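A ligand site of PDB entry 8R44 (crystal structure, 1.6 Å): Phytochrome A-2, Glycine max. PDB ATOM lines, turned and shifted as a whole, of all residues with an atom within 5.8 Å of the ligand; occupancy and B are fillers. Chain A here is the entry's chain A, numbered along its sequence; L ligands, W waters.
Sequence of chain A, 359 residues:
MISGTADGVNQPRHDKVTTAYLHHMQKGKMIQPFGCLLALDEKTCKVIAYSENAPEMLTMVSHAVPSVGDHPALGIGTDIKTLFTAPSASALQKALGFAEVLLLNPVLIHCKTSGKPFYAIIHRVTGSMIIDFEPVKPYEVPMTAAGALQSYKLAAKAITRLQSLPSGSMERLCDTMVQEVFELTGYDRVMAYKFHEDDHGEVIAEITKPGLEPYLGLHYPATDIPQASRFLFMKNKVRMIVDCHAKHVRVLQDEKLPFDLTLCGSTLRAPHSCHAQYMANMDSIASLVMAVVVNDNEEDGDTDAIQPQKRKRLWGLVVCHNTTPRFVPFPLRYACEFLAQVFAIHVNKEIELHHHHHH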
ATOM      1  N   TYR A  21      -5.969 -25.672  14.721  1.00  0.00           N
ATOM      2  CA  TYR A  21      -5.873 -24.523  15.607  1.00  0.00           C
ATOM      3  C   TYR A  21      -4.754 -23.584  15.158  1.00  0.00           C
ATOM      4  O   TYR A  21      -4.977 -22.387  14.987  1.00  0.00           O
ATOM      5  CB  TYR A  21      -5.597 -24.920  17.061  1.00  0.00           C
ATOM      6  CG  TYR A  21      -6.808 -25.212  17.898  1.00  0.00           C
ATOM      7  CD1 TYR A  21      -7.881 -24.334  17.952  1.00  0.00           C
ATOM      8  CD2 TYR A  21      -6.866 -26.359  18.689  1.00  0.00           C
ATOM      9  CE1 TYR A  21      -8.991 -24.601  18.738  1.00  0.00           C
ATOM     10  CE2 TYR A  21      -7.966 -26.629  19.478  1.00  0.00           C
ATOM     11  CZ  TYR A  21      -9.040 -25.743  19.509  1.00  0.00           C
ATOM     12  OH  TYR A  21     -10.122 -26.025  20.298  1.00  0.00           O
ATOM     13  N   MET A  25      -4.526 -19.565  13.285  1.00  0.00           N
ATOM     14  CA  MET A  25      -3.926 -18.616  14.232  1.00  0.00           C
ATOM     15  C   MET A  25      -2.622 -18.092  13.634  1.00  0.00           C
ATOM     16  O   MET A  25      -2.182 -16.997  13.995  1.00  0.00           O
ATOM     17  CB  MET A  25      -3.601 -19.282  15.579  1.00  0.00           C
ATOM     18  CG  MET A  25      -4.686 -19.122  16.642  1.00  0.00           C
ATOM     19  SD  MET A  25      -4.125 -19.632  18.289  1.00  0.00           S
ATOM     20  CE  MET A  25      -5.363 -20.882  18.667  1.00  0.00           C
ATOM     21  N   MET A 191      -7.490 -12.117  37.549  1.00  0.00           N
ATOM     22  CA  MET A 191      -7.205 -13.442  38.063  1.00  0.00           C
ATOM     23  C   MET A 191      -5.756 -13.801  37.738  1.00  0.00           C
ATOM     24  O   MET A 191      -5.222 -13.448  36.689  1.00  0.00           O
ATOM     25  CB  MET A 191      -8.097 -14.500  37.423  1.00  0.00           C
ATOM     26  CG  MET A 191      -9.553 -14.343  37.729  1.00  0.00           C
ATOM     27  SD  MET A 191     -10.621 -15.418  36.763  1.00  0.00           S
ATOM     28  CE  MET A 191     -10.563 -14.654  35.125  1.00  0.00           C
ATOM     29  N   TYR A 193      -3.929 -17.221  36.899  1.00  0.00           N
ATOM     30  CA  TYR A 193      -4.311 -18.519  36.392  1.00  0.00           C
ATOM     31  C   TYR A 193      -3.057 -19.364  36.193  1.00  0.00           C
ATOM     32  O   TYR A 193      -2.252 -19.098  35.307  1.00  0.00           O
ATOM     33  CB  TYR A 193      -5.064 -18.330  35.062  1.00  0.00           C
ATOM     34  CG  TYR A 193      -5.714 -19.559  34.469  1.00  0.00           C
ATOM     35  CD1 TYR A 193      -6.942 -20.006  34.915  1.00  0.00           C
ATOM     36  CD2 TYR A 193      -5.099 -20.265  33.453  1.00  0.00           C
ATOM     37  CE1 TYR A 193      -7.539 -21.134  34.377  1.00  0.00           C
ATOM     38  CE2 TYR A 193      -5.687 -21.388  32.895  1.00  0.00           C
ATOM     39  CZ  TYR A 193      -6.939 -21.805  33.338  1.00  0.00           C
ATOM     40  OH  TYR A 193      -7.506 -22.912  32.764  1.00  0.00           O
ATOM     41  N   VAL A 203      -7.456 -21.067  39.020  1.00  0.00           N
ATOM     42  CA  VAL A 203      -7.487 -19.681  39.459  1.00  0.00           C
ATOM     43  C   VAL A 203      -6.961 -19.619  40.890  1.00  0.00           C
ATOM     44  O   VAL A 203      -7.681 -20.049  41.809  1.00  0.00           O
ATOM     45  CB  VAL A 203      -8.888 -19.083  39.373  1.00  0.00           C
ATOM     46  CG1 VAL A 203      -8.851 -17.613  39.843  1.00  0.00           C
ATOM     47  CG2 VAL A 203      -9.480 -19.259  37.972  1.00  0.00           C
ATOM     48  N   TYR A 215     -14.515 -16.517  40.708  1.00  0.00           N
ATOM     49  CA  TYR A 215     -13.996 -17.742  40.136  1.00  0.00           C
ATOM     50  C   TYR A 215     -12.817 -18.288  40.929  1.00  0.00           C
ATOM     51  O   TYR A 215     -12.279 -19.340  40.568  1.00  0.00           O
ATOM     52  CB  TYR A 215     -13.509 -17.478  38.711  1.00  0.00           C
ATOM     53  CG  TYR A 215     -14.633 -17.070  37.804  1.00  0.00           C
ATOM     54  CD1 TYR A 215     -15.915 -17.533  38.046  1.00  0.00           C
ATOM     55  CD2 TYR A 215     -14.466 -16.160  36.789  1.00  0.00           C
ATOM     56  CE1 TYR A 215     -16.987 -17.164  37.241  1.00  0.00           C
ATOM     57  CE2 TYR A 215     -15.526 -15.751  36.014  1.00  0.00           C
ATOM     58  CZ  TYR A 215     -16.789 -16.256  36.229  1.00  0.00           C
ATOM     59  OH  TYR A 215     -17.842 -15.907  35.446  1.00  0.00           O
ATOM     60  N   TYR A 220      -9.791 -25.778  35.654  1.00  0.00           N
ATOM     61  CA  TYR A 220     -10.321 -25.856  34.312  1.00  0.00           C
ATOM     62  C   TYR A 220      -9.459 -26.804  33.491  1.00  0.00           C
ATOM     63  O   TYR A 220      -8.258 -26.895  33.715  1.00  0.00           O
ATOM     64  CB  TYR A 220     -10.309 -24.492  33.610  1.00  0.00           C
ATOM     65  CG  TYR A 220     -11.287 -23.483  34.158  1.00  0.00           C
ATOM     66  CD1 TYR A 220     -10.928 -22.728  35.254  1.00  0.00           C
ATOM     67  CD2 TYR A 220     -12.578 -23.354  33.655  1.00  0.00           C
ATOM     68  CE1 TYR A 220     -11.795 -21.786  35.776  1.00  0.00           C
ATOM     69  CE2 TYR A 220     -13.475 -22.448  34.199  1.00  0.00           C
ATOM     70  CZ  TYR A 220     -13.076 -21.682  35.286  1.00  0.00           C
ATOM     71  OH  TYR A 220     -13.828 -20.715  35.873  1.00  0.00           O
ATOM     72  N   PRO A 221     -10.061 -27.524  32.520  1.00  0.00           N
ATOM     73  CA  PRO A 221      -9.341 -28.507  31.729  1.00  0.00           C
ATOM     74  C   PRO A 221      -8.293 -27.831  30.857  1.00  0.00           C
ATOM     75  O   PRO A 221      -8.478 -26.698  30.434  1.00  0.00           O
ATOM     76  CB  PRO A 221     -10.384 -29.179  30.833  1.00  0.00           C
ATOM     77  CG  PRO A 221     -11.663 -28.385  30.967  1.00  0.00           C
ATOM     78  CD  PRO A 221     -11.478 -27.443  32.150  1.00  0.00           C
ATOM     79  N   THR A 223      -7.705 -28.366  27.864  1.00  0.00           N
ATOM     80  CA  THR A 223      -8.166 -28.103  26.514  1.00  0.00           C
ATOM     81  C   THR A 223      -8.806 -26.710  26.379  1.00  0.00           C
ATOM     82  O   THR A 223      -9.011 -26.245  25.248  1.00  0.00           O
ATOM     83  CB  THR A 223      -9.080 -29.232  26.036  1.00  0.00           C
ATOM     84  OG1 THR A 223     -10.058 -29.402  27.060  1.00  0.00           O
ATOM     85  CG2 THR A 223      -8.323 -30.525  25.793  1.00  0.00           C
ATOM     86  N   ASP A 224      -9.171 -26.054  27.489  1.00  0.00           N
ATOM     87  CA  ASP A 224      -9.718 -24.710  27.394  1.00  0.00           C
ATOM     88  C   ASP A 224      -8.692 -23.741  26.794  1.00  0.00           C
ATOM     89  O   ASP A 224      -9.082 -22.737  26.193  1.00  0.00           O
ATOM     90  CB  ASP A 224     -10.207 -24.164  28.733  1.00  0.00           C
ATOM     91  CG  ASP A 224     -11.546 -24.727  29.179  1.00  0.00           C
ATOM     92  OD1 ASP A 224     -11.997 -25.711  28.598  1.00  0.00           O
ATOM     93  OD2 ASP A 224     -12.150 -24.154  30.089  1.00  0.00           O
ATOM     94  N   ILE A 225      -7.396 -23.998  27.053  1.00  0.00           N
ATOM     95  CA  ILE A 225      -6.335 -23.187  26.475  1.00  0.00           C
ATOM     96  C   ILE A 225      -5.443 -24.121  25.670  1.00  0.00           C
ATOM     97  O   ILE A 225      -4.548 -24.751  26.234  1.00  0.00           O
ATOM     98  CB  ILE A 225      -5.536 -22.377  27.520  1.00  0.00           C
ATOM     99  CG1 ILE A 225      -6.489 -21.634  28.467  1.00  0.00           C
ATOM    100  CG2 ILE A 225      -4.582 -21.407  26.813  1.00  0.00           C
ATOM    101  CD1 ILE A 225      -5.822 -20.606  29.348  1.00  0.00           C
ATOM    102  N   PRO A 226      -5.697 -24.248  24.349  1.00  0.00           N
ATOM    103  CA  PRO A 226      -4.940 -25.158  23.482  1.00  0.00           C
ATOM    104  C   PRO A 226      -3.448 -24.832  23.468  1.00  0.00           C
ATOM    105  O   PRO A 226      -3.046 -23.694  23.724  1.00  0.00           O
ATOM    106  CB  PRO A 226      -5.499 -24.932  22.066  1.00  0.00           C
ATOM    107  CG  PRO A 226      -6.811 -24.189  22.252  1.00  0.00           C
ATOM    108  CD  PRO A 226      -6.738 -23.499  23.610  1.00  0.00           C
ATOM    109  N   SER A 229      -2.194 -21.782  21.576  1.00  0.00           N
ATOM    110  CA  SER A 229      -2.386 -20.534  22.299  1.00  0.00           C
ATOM    111  C   SER A 229      -1.326 -20.370  23.385  1.00  0.00           C
ATOM    112  O   SER A 229      -0.788 -19.276  23.562  1.00  0.00           O
ATOM    113  CB  SER A 229      -3.783 -20.465  22.833  1.00  0.00           C
ATOM    114  OG  SER A 229      -4.704 -20.557  21.751  1.00  0.00           O
ATOM    115  N   LEU A 232       1.877 -19.454  21.702  1.00  0.00           N
ATOM    116  CA  LEU A 232       1.925 -18.077  21.250  1.00  0.00           C
ATOM    117  C   LEU A 232       2.294 -17.142  22.405  1.00  0.00           C
ATOM    118  O   LEU A 232       2.980 -16.131  22.182  1.00  0.00           O
ATOM    119  CB  LEU A 232       0.581 -17.702  20.630  1.00  0.00           C
ATOM    120  CG  LEU A 232       0.416 -16.271  20.112  1.00  0.00           C
ATOM    121  CD1 LEU A 232      -0.588 -16.229  18.970  1.00  0.00           C
ATOM    122  CD2 LEU A 232      -0.015 -15.288  21.207  1.00  0.00           C
ATOM    123  N   PHE A 233       1.760 -17.410  23.613  1.00  0.00           N
ATOM    124  CA  PHE A 233       1.988 -16.531  24.747  1.00  0.00           C
ATOM    125  C   PHE A 233       3.473 -16.446  25.091  1.00  0.00           C
ATOM    126  O   PHE A 233       3.912 -15.474  25.699  1.00  0.00           O
ATOM    127  CB  PHE A 233       1.146 -16.985  25.933  1.00  0.00           C
ATOM    128  CG  PHE A 233      -0.260 -16.445  25.908  1.00  0.00           C
ATOM    129  CD1 PHE A 233      -0.477 -15.084  25.855  1.00  0.00           C
ATOM    130  CD2 PHE A 233      -1.360 -17.286  25.976  1.00  0.00           C
ATOM    131  CE1 PHE A 233      -1.770 -14.576  25.825  1.00  0.00           C
ATOM    132  CE2 PHE A 233      -2.647 -16.787  25.986  1.00  0.00           C
ATOM    133  CZ  PHE A 233      -2.842 -15.416  25.879  1.00  0.00           C
ATOM    134  N   ARG A 239      -2.078  -9.742  25.308  1.00  0.00           N
ATOM    135  CA  ARG A 239      -3.123  -9.941  24.304  1.00  0.00           C
ATOM    136  C   ARG A 239      -4.391  -9.239  24.799  1.00  0.00           C
ATOM    137  O   ARG A 239      -4.839  -9.515  25.916  1.00  0.00           O
ATOM    138  CB  ARG A 239      -3.373 -11.422  24.055  1.00  0.00           C
ATOM    139  CG  ARG A 239      -4.050 -11.768  22.728  1.00  0.00           C
ATOM    140  CD  ARG A 239      -5.514 -11.417  22.652  1.00  0.00           C
ATOM    141  NE  ARG A 239      -6.011 -11.533  21.279  1.00  0.00           N
ATOM    142  CZ  ARG A 239      -6.310 -12.684  20.722  1.00  0.00           C
ATOM    143  NH1 ARG A 239      -6.156 -13.794  21.439  1.00  0.00           N
ATOM    144  NH2 ARG A 239      -6.822 -12.733  19.511  1.00  0.00           N
ATOM    145  N   ILE A 241      -8.500  -8.234  23.878  1.00  0.00           N
ATOM    146  CA  ILE A 241      -9.720  -8.382  23.104  1.00  0.00           C
ATOM    147  C   ILE A 241     -10.705  -7.334  23.639  1.00  0.00           C
ATOM    148  O   ILE A 241     -11.104  -7.346  24.799  1.00  0.00           O
ATOM    149  CB  ILE A 241     -10.302  -9.808  23.189  1.00  0.00           C
ATOM    150  CG1 ILE A 241      -9.322 -10.847  22.674  1.00  0.00           C
ATOM    151  CG2 ILE A 241     -11.664  -9.883  22.535  1.00  0.00           C
ATOM    152  CD1 ILE A 241      -9.696 -12.264  23.021  1.00  0.00           C
ATOM    153  N   ARG A 269      -5.090  -8.970  16.242  1.00  0.00           N
ATOM    154  CA  ARG A 269      -5.525 -10.284  15.779  1.00  0.00           C
ATOM    155  C   ARG A 269      -6.881 -10.647  16.407  1.00  0.00           C
ATOM    156  O   ARG A 269      -7.045 -10.512  17.613  1.00  0.00           O
ATOM    157  CB  ARG A 269      -4.454 -11.310  16.114  1.00  0.00           C
ATOM    158  CG  ARG A 269      -4.865 -12.727  15.687  1.00  0.00           C
ATOM    159  CD  ARG A 269      -3.731 -13.715  15.839  1.00  0.00           C
ATOM    160  NE  ARG A 269      -3.382 -13.882  17.243  1.00  0.00           N
ATOM    161  CZ  ARG A 269      -4.062 -14.674  18.065  1.00  0.00           C
ATOM    162  NH1 ARG A 269      -5.063 -15.397  17.605  1.00  0.00           N
ATOM    163  NH2 ARG A 269      -3.750 -14.732  19.351  1.00  0.00           N
ATOM    164  N   ALA A 270      -7.839 -11.118  15.593  1.00  0.00           N
ATOM    165  CA  ALA A 270      -9.175 -11.483  16.065  1.00  0.00           C
ATOM    166  C   ALA A 270      -9.100 -12.764  16.871  1.00  0.00           C
ATOM    167  O   ALA A 270      -8.284 -13.617  16.633  1.00  0.00           O
ATOM    168  CB  ALA A 270     -10.140 -11.672  14.907  1.00  0.00           C
ATOM    169  N   PRO A 271      -9.936 -12.915  17.911  1.00  0.00           N
ATOM    170  CA  PRO A 271      -9.984 -14.196  18.626  1.00  0.00           C
ATOM    171  C   PRO A 271     -10.623 -15.237  17.717  1.00  0.00           C
ATOM    172  O   PRO A 271     -11.575 -14.911  17.007  1.00  0.00           O
ATOM    173  CB  PRO A 271     -10.832 -13.892  19.854  1.00  0.00           C
ATOM    174  CG  PRO A 271     -11.652 -12.686  19.485  1.00  0.00           C
ATOM    175  CD  PRO A 271     -10.824 -11.917  18.474  1.00  0.00           C
ATOM    176  N   HIS A 272     -10.148 -16.480  17.788  1.00  0.00           N
ATOM    177  CA  HIS A 272     -10.833 -17.634  17.201  1.00  0.00           C
ATOM    178  C   HIS A 272     -12.299 -17.639  17.620  1.00  0.00           C
ATOM    179  O   HIS A 272     -12.613 -17.284  18.745  1.00  0.00           O
ATOM    180  CB  HIS A 272     -10.117 -18.908  17.623  1.00  0.00           C
ATOM    181  CG  HIS A 272     -10.593 -20.140  16.938  1.00  0.00           C
ATOM    182  ND1 HIS A 272     -11.825 -20.719  17.160  1.00  0.00           N
ATOM    183  CD2 HIS A 272      -9.959 -20.934  16.046  1.00  0.00           C
ATOM    184  CE1 HIS A 272     -11.945 -21.821  16.413  1.00  0.00           C
ATOM    185  NE2 HIS A 272     -10.823 -21.964  15.726  1.00  0.00           N
ATOM    186  N   CYS A 274     -14.321 -19.883  18.389  1.00  0.00           N
ATOM    187  CA  CYS A 274     -14.579 -20.748  19.543  1.00  0.00           C
ATOM    188  C   CYS A 274     -14.405 -19.924  20.820  1.00  0.00           C
ATOM    189  O   CYS A 274     -15.272 -19.937  21.683  1.00  0.00           O
ATOM    190  CB  CYS A 274     -13.670 -21.973  19.644  1.00  0.00           C
ATOM    191  SG  CYS A 274     -13.993 -23.019  21.117  1.00  0.00           S
ATOM    192  N   HIS A 275     -13.282 -19.196  20.902  1.00  0.00           N
ATOM    193  CA  HIS A 275     -12.989 -18.425  22.110  1.00  0.00           C
ATOM    194  C   HIS A 275     -13.935 -17.224  22.252  1.00  0.00           C
ATOM    195  O   HIS A 275     -14.375 -16.885  23.345  1.00  0.00           O
ATOM    196  CB  HIS A 275     -11.530 -17.966  22.143  1.00  0.00           C
ATOM    197  CG  HIS A 275     -11.224 -17.207  23.394  1.00  0.00           C
ATOM    198  ND1 HIS A 275     -11.270 -17.803  24.636  1.00  0.00           N
ATOM    199  CD2 HIS A 275     -10.858 -15.904  23.604  1.00  0.00           C
ATOM    200  CE1 HIS A 275     -10.942 -16.895  25.570  1.00  0.00           C
ATOM    201  NE2 HIS A 275     -10.682 -15.735  24.965  1.00  0.00           N
ATOM    202  N   TYR A 278     -16.832 -18.620  23.861  1.00  0.00           N
ATOM    203  CA  TYR A 278     -16.500 -18.892  25.258  1.00  0.00           C
ATOM    204  C   TYR A 278     -16.607 -17.619  26.105  1.00  0.00           C
ATOM    205  O   TYR A 278     -17.059 -17.652  27.242  1.00  0.00           O
ATOM    206  CB  TYR A 278     -15.075 -19.431  25.326  1.00  0.00           C
ATOM    207  CG  TYR A 278     -14.592 -19.963  26.642  1.00  0.00           C
ATOM    208  CD1 TYR A 278     -13.886 -19.175  27.530  1.00  0.00           C
ATOM    209  CD2 TYR A 278     -14.750 -21.307  26.966  1.00  0.00           C
ATOM    210  CE1 TYR A 278     -13.396 -19.677  28.727  1.00  0.00           C
ATOM    211  CE2 TYR A 278     -14.277 -21.827  28.166  1.00  0.00           C
ATOM    212  CZ  TYR A 278     -13.587 -21.012  29.055  1.00  0.00           C
ATOM    213  OH  TYR A 278     -13.091 -21.524  30.261  1.00  0.00           O
ATOM    214  N   MET A 282     -19.333 -16.675  29.206  1.00  0.00           N
ATOM    215  CA  MET A 282     -19.042 -16.385  30.618  1.00  0.00           C
ATOM    216  C   MET A 282     -19.129 -14.885  30.934  1.00  0.00           C
ATOM    217  O   MET A 282     -18.749 -14.451  32.023  1.00  0.00           O
ATOM    218  CB  MET A 282     -17.720 -16.971  31.126  1.00  0.00           C
ATOM    219  CG  MET A 282     -16.467 -16.504  30.441  1.00  0.00           C
ATOM    220  SD  MET A 282     -14.968 -17.285  31.192  1.00  0.00           S
ATOM    221  CE  MET A 282     -14.973 -16.587  32.844  1.00  0.00           C
ATOM    222  N   SER A 287     -11.219  -8.717  27.356  1.00  0.00           N
ATOM    223  CA  SER A 287     -10.163  -9.302  28.156  1.00  0.00           C
ATOM    224  C   SER A 287      -8.819  -8.634  27.875  1.00  0.00           C
ATOM    225  O   SER A 287      -8.588  -8.137  26.776  1.00  0.00           O
ATOM    226  CB  SER A 287     -10.058 -10.809  27.937  1.00  0.00           C
ATOM    227  OG  SER A 287      -9.844 -11.153  26.576  1.00  0.00           O
ATOM    228  N   VAL A 289      -4.855 -10.176  28.644  1.00  0.00           N
ATOM    229  CA  VAL A 289      -4.139 -11.328  29.169  1.00  0.00           C
ATOM    230  C   VAL A 289      -2.634 -11.085  29.083  1.00  0.00           C
ATOM    231  O   VAL A 289      -2.091 -10.734  28.007  1.00  0.00           O
ATOM    232  CB  VAL A 289      -4.604 -12.606  28.446  1.00  0.00           C
ATOM    233  CG1 VAL A 289      -3.849 -13.862  28.865  1.00  0.00           C
ATOM    234  CG2 VAL A 289      -6.097 -12.817  28.586  1.00  0.00           C
ATOM    235  N   LEU A 317      -1.016 -17.212  33.511  1.00  0.00           N
ATOM    236  CA  LEU A 317      -1.507 -15.996  32.869  1.00  0.00           C
ATOM    237  C   LEU A 317      -2.095 -15.093  33.941  1.00  0.00           C
ATOM    238  O   LEU A 317      -2.732 -15.577  34.890  1.00  0.00           O
ATOM    239  CB  LEU A 317      -2.590 -16.323  31.839  1.00  0.00           C
ATOM    240  CG  LEU A 317      -2.259 -17.360  30.766  1.00  0.00           C
ATOM    241  CD1 LEU A 317      -3.485 -17.741  29.976  1.00  0.00           C
ATOM    242  CD2 LEU A 317      -1.195 -16.819  29.834  1.00  0.00           C
ATOM    243  N   VAL A 319      -5.102 -12.735  33.926  1.00  0.00           N
ATOM    244  CA  VAL A 319      -6.266 -12.684  33.059  1.00  0.00           C
ATOM    245  C   VAL A 319      -7.164 -11.580  33.612  1.00  0.00           C
ATOM    246  O   VAL A 319      -7.652 -11.675  34.741  1.00  0.00           O
ATOM    247  CB  VAL A 319      -7.005 -14.025  33.004  1.00  0.00           C
ATOM    248  CG1 VAL A 319      -8.238 -13.933  32.120  1.00  0.00           C
ATOM    249  CG2 VAL A 319      -6.131 -15.168  32.521  1.00  0.00           C
ATOM    250  N   HIS A 321     -10.728  -9.527  32.903  1.00  0.00           N
ATOM    251  CA  HIS A 321     -11.998  -9.575  32.196  1.00  0.00           C
ATOM    252  C   HIS A 321     -12.853  -8.367  32.524  1.00  0.00           C
ATOM    253  O   HIS A 321     -12.797  -7.821  33.624  1.00  0.00           O
ATOM    254  CB  HIS A 321     -12.816 -10.788  32.628  1.00  0.00           C
ATOM    255  CG  HIS A 321     -12.321 -12.076  32.164  1.00  0.00           C
ATOM    256  ND1 HIS A 321     -12.956 -13.181  32.665  1.00  0.00           N
ATOM    257  CD2 HIS A 321     -11.464 -12.500  31.283  1.00  0.00           C
ATOM    258  CE1 HIS A 321     -12.409 -14.238  32.120  1.00  0.00           C
ATOM    259  NE2 HIS A 321     -11.507 -13.868  31.258  1.00  0.00           N
HETATM  260  C1  LIG L   1      -7.918 -19.060  24.317  1.00  0.00           C
HETATM  261  N1  LIG L   1      -8.937 -19.707  26.442  1.00  0.00           N
HETATM  262  C2  LIG L   1      -8.040 -18.941  25.701  1.00  0.00           C
HETATM  263  C3  LIG L   1      -7.422 -17.929  26.552  1.00  0.00           C
HETATM  264  C4  LIG L   1      -7.948 -18.077  27.837  1.00  0.00           C
HETATM  265  C5  LIG L   1      -8.894 -19.214  27.758  1.00  0.00           C
HETATM  266  C6  LIG L   1      -7.591 -17.243  29.069  1.00  0.00           C
HETATM  267  C7  LIG L   1      -6.412 -16.886  26.091  1.00  0.00           C
HETATM  268  C8  LIG L   1      -7.217 -15.971  25.157  1.00  0.00           C
HETATM  269  C9  LIG L   1      -6.616 -14.590  24.857  1.00  0.00           C
HETATM  270  O1  LIG L   1      -5.778 -14.553  23.968  1.00  0.00           O
HETATM  271  O2  LIG L   1      -7.080 -13.651  25.415  1.00  0.00           O
HETATM  272  C10 LIG L   1      -9.678 -19.783  28.807  1.00  0.00           C
HETATM  273  N2  LIG L   1     -10.185 -17.875  30.188  1.00  0.00           N
HETATM  274  C11 LIG L   1     -10.041 -19.255  30.024  1.00  0.00           C
HETATM  275  C12 LIG L   1     -10.324 -19.969  31.249  1.00  0.00           C
HETATM  276  C13 LIG L   1     -10.652 -19.004  32.223  1.00  0.00           C
HETATM  277  C14 LIG L   1     -10.545 -17.659  31.516  1.00  0.00           C
HETATM  278  C15 LIG L   1     -10.232 -21.496  31.429  1.00  0.00           C
HETATM  279  C16 LIG L   1     -11.002 -19.051  33.715  1.00  0.00           C
HETATM  280  C17 LIG L   1     -12.322 -18.390  34.047  1.00  0.00           C
HETATM  281  O3  LIG L   1     -10.766 -16.580  31.966  1.00  0.00           O
HETATM  282  N3  LIG L   1     -11.697 -23.126  24.063  1.00  0.00           N
HETATM  283  C18 LIG L   1     -12.713 -23.963  24.554  1.00  0.00           C
HETATM  284  C19 LIG L   1     -13.019 -25.051  23.535  1.00  0.00           C
HETATM  285  C20 LIG L   1     -12.081 -24.718  22.322  1.00  0.00           C
HETATM  286  C21 LIG L   1     -11.215 -23.540  22.818  1.00  0.00           C
HETATM  287  C22 LIG L   1     -13.037 -26.491  24.128  1.00  0.00           C
HETATM  288  C23 LIG L   1     -12.813 -24.425  20.985  1.00  0.00           C
HETATM  289  C24 LIG L   1     -13.427 -25.656  20.351  1.00  0.00           C
HETATM  290  O4  LIG L   1     -13.300 -23.803  25.640  1.00  0.00           O
HETATM  291  C25 LIG L   1     -10.312 -22.893  22.057  1.00  0.00           C
HETATM  292  N4  LIG L   1      -9.296 -21.081  23.522  1.00  0.00           N
HETATM  293  C26 LIG L   1      -9.509 -21.728  22.317  1.00  0.00           C
HETATM  294  C27 LIG L   1      -8.759 -21.018  21.322  1.00  0.00           C
HETATM  295  C28 LIG L   1      -8.095 -19.970  21.977  1.00  0.00           C
HETATM  296  C29 LIG L   1      -8.424 -19.991  23.370  1.00  0.00           C
HETATM  297  C30 LIG L   1      -8.684 -21.371  19.849  1.00  0.00           C
HETATM  298  C31 LIG L   1      -7.161 -18.939  21.379  1.00  0.00           C
HETATM  299  C32 LIG L   1      -7.984 -17.780  20.885  1.00  0.00           C
HETATM  300  C33 LIG L   1      -7.105 -16.853  20.045  1.00  0.00           C
HETATM  301  O5  LIG L   1      -5.979 -16.567  20.480  1.00  0.00           O
HETATM  302  O6  LIG L   1      -7.615 -16.473  18.992  1.00  0.00           O
HETATM  303  O   HOH W   1      -9.604 -13.886  26.597  1.00  0.00           O
HETATM  304  O   HOH W   2     -11.522 -20.540  25.368  1.00  0.00           O
HETATM  305  O   HOH W   3      -4.582 -16.776  22.807  1.00  0.00           O
HETATM  306  O   HOH W   4      -7.309 -11.024  25.711  1.00  0.00           O
HETATM  307  O   HOH W   5     -10.437 -15.270  28.842  1.00  0.00           O
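Water W4 lies within hydrogen-bond range of an oxygen (O2) of the ligand (2.7 Å), the side-chain hydroxyl of Ser 287 (2.7 Å) and the backbone carbonyl oxygen of Arg 239 (2.9 Å).
Water W1 lies within hydrogen-bond range of NE2 of His 275, OG of Ser 287 and O2 of the ligand.
Water W2 lies within hydrogen-bond range of a ring nitrogen (ND1) of His 275, a nitrogen (N3) of the ligand and the backbone carbonyl oxygen of Asp 224.
Water W5 bridges N2 of the ligand (2.9 Å) and NE2 of His 321 (3.0 Å).
The backbone NH (N) of Cys 274 is in hydrogen-bond range of a ring nitrogen (ND1) of His 272 (2.9 Å).
The guanidinium group (NH2) of Arg 239 is in hydrogen-bond range of the backbone carbonyl oxygen (O) of Arg 269 (2.9 Å).
The backbone carbonyl oxygen (O) of Ala 270 sits at hydrogen-bond distance from the guanidinium group (NH2) of Arg 239 (3.3 Å).
The side-chain hydroxyl of Ser 229 sits close to the side-chain sulfur of Met 25.
The side-chain carboxylate (OD2) of Asp 224 sits at hydrogen-bond distance from the side-chain hydroxyl (OH) of Tyr 278.
O of Leu 317 lies within hydrogen-bond range of N of Tyr 193 (2.9 Å).
The backbone carbonyl oxygen (O) of Val 319 sits at hydrogen-bond distance from the backbone NH (N) of Met 191 (2.8 Å).
O of Ser 287 sits at hydrogen-bond distance from N of Ile 241, at 2.9 Å.
Tyr 21 touches the ligand (OH to C20, 3.1 Å).
CE of Met 25 touches C30 of the ligand, at 3.6 Å.
CE of Met 191 touches O3 of the ligand, at 3.7 Å.
OH of Tyr 193 touches C15 of the ligand, 3.3 Å away.
OH of Tyr 220 touches C17 of the ligand (3.3 Å).
Ile 225 touches the ligand.
CD of Pro 226 touches N4 of the ligand, 3.5 Å away.
Ser 229 touches the ligand (OG to C31, 3.0 Å).
Phe 233 touches the ligand (CZ to O1, 3.6 Å).
Ile 241 touches the ligand (CD1 to O2, 3.8 Å).
Ala 270 touches the ligand.
Pro 271 touches the ligand.
NE2 of His 275 touches C8 of the ligand, at 3.5 Å.
Tyr 278 touches the ligand (OH to C15, 3.1 Å).
CE of Met 282 touches C17 of the ligand (3.4 Å).
Ser 287 touches the ligand (OG to O2, 3.9 Å).
CG2 of Val 289 touches O2 of the ligand, 3.4 Å away.
Val 319 touches the ligand.
Hydrophobic or aromatic side chains within 4 Å of the ligand: Tyr 21, Met 25, Met 191, Tyr 193, Tyr 220, Ile 225, Pro 226, Phe 233, Ile 241, His 272, His 275, Tyr 278, Met 282, Val 289, Val 319 and His 321.
The nearest printed residue that does not touch the ligand is Tyr 215 (4.1 Å).
The side-chain sulfur (SG) of Cys 274 is covalently linked to a carbon (C23) of the ligand, at 1.8 Å.
An oxygen (O1) of the ligand lies within salt-bridge range of the guanidinium group (NH1) of Arg 239.
N of His 272 is in hydrogen-bond range of O6 of the ligand (2.8 Å).
An oxygen (O3) of the ligand lies close to a ring nitrogen (NE2) of His 321 (2.9 Å).
N4 of the ligand sits at hydrogen-bond distance from O of Asp 224 (3.1 Å).
An oxygen (O6) of the ligand is in salt-bridge range of the guanidinium group of Arg 269, 3.1 Å away.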
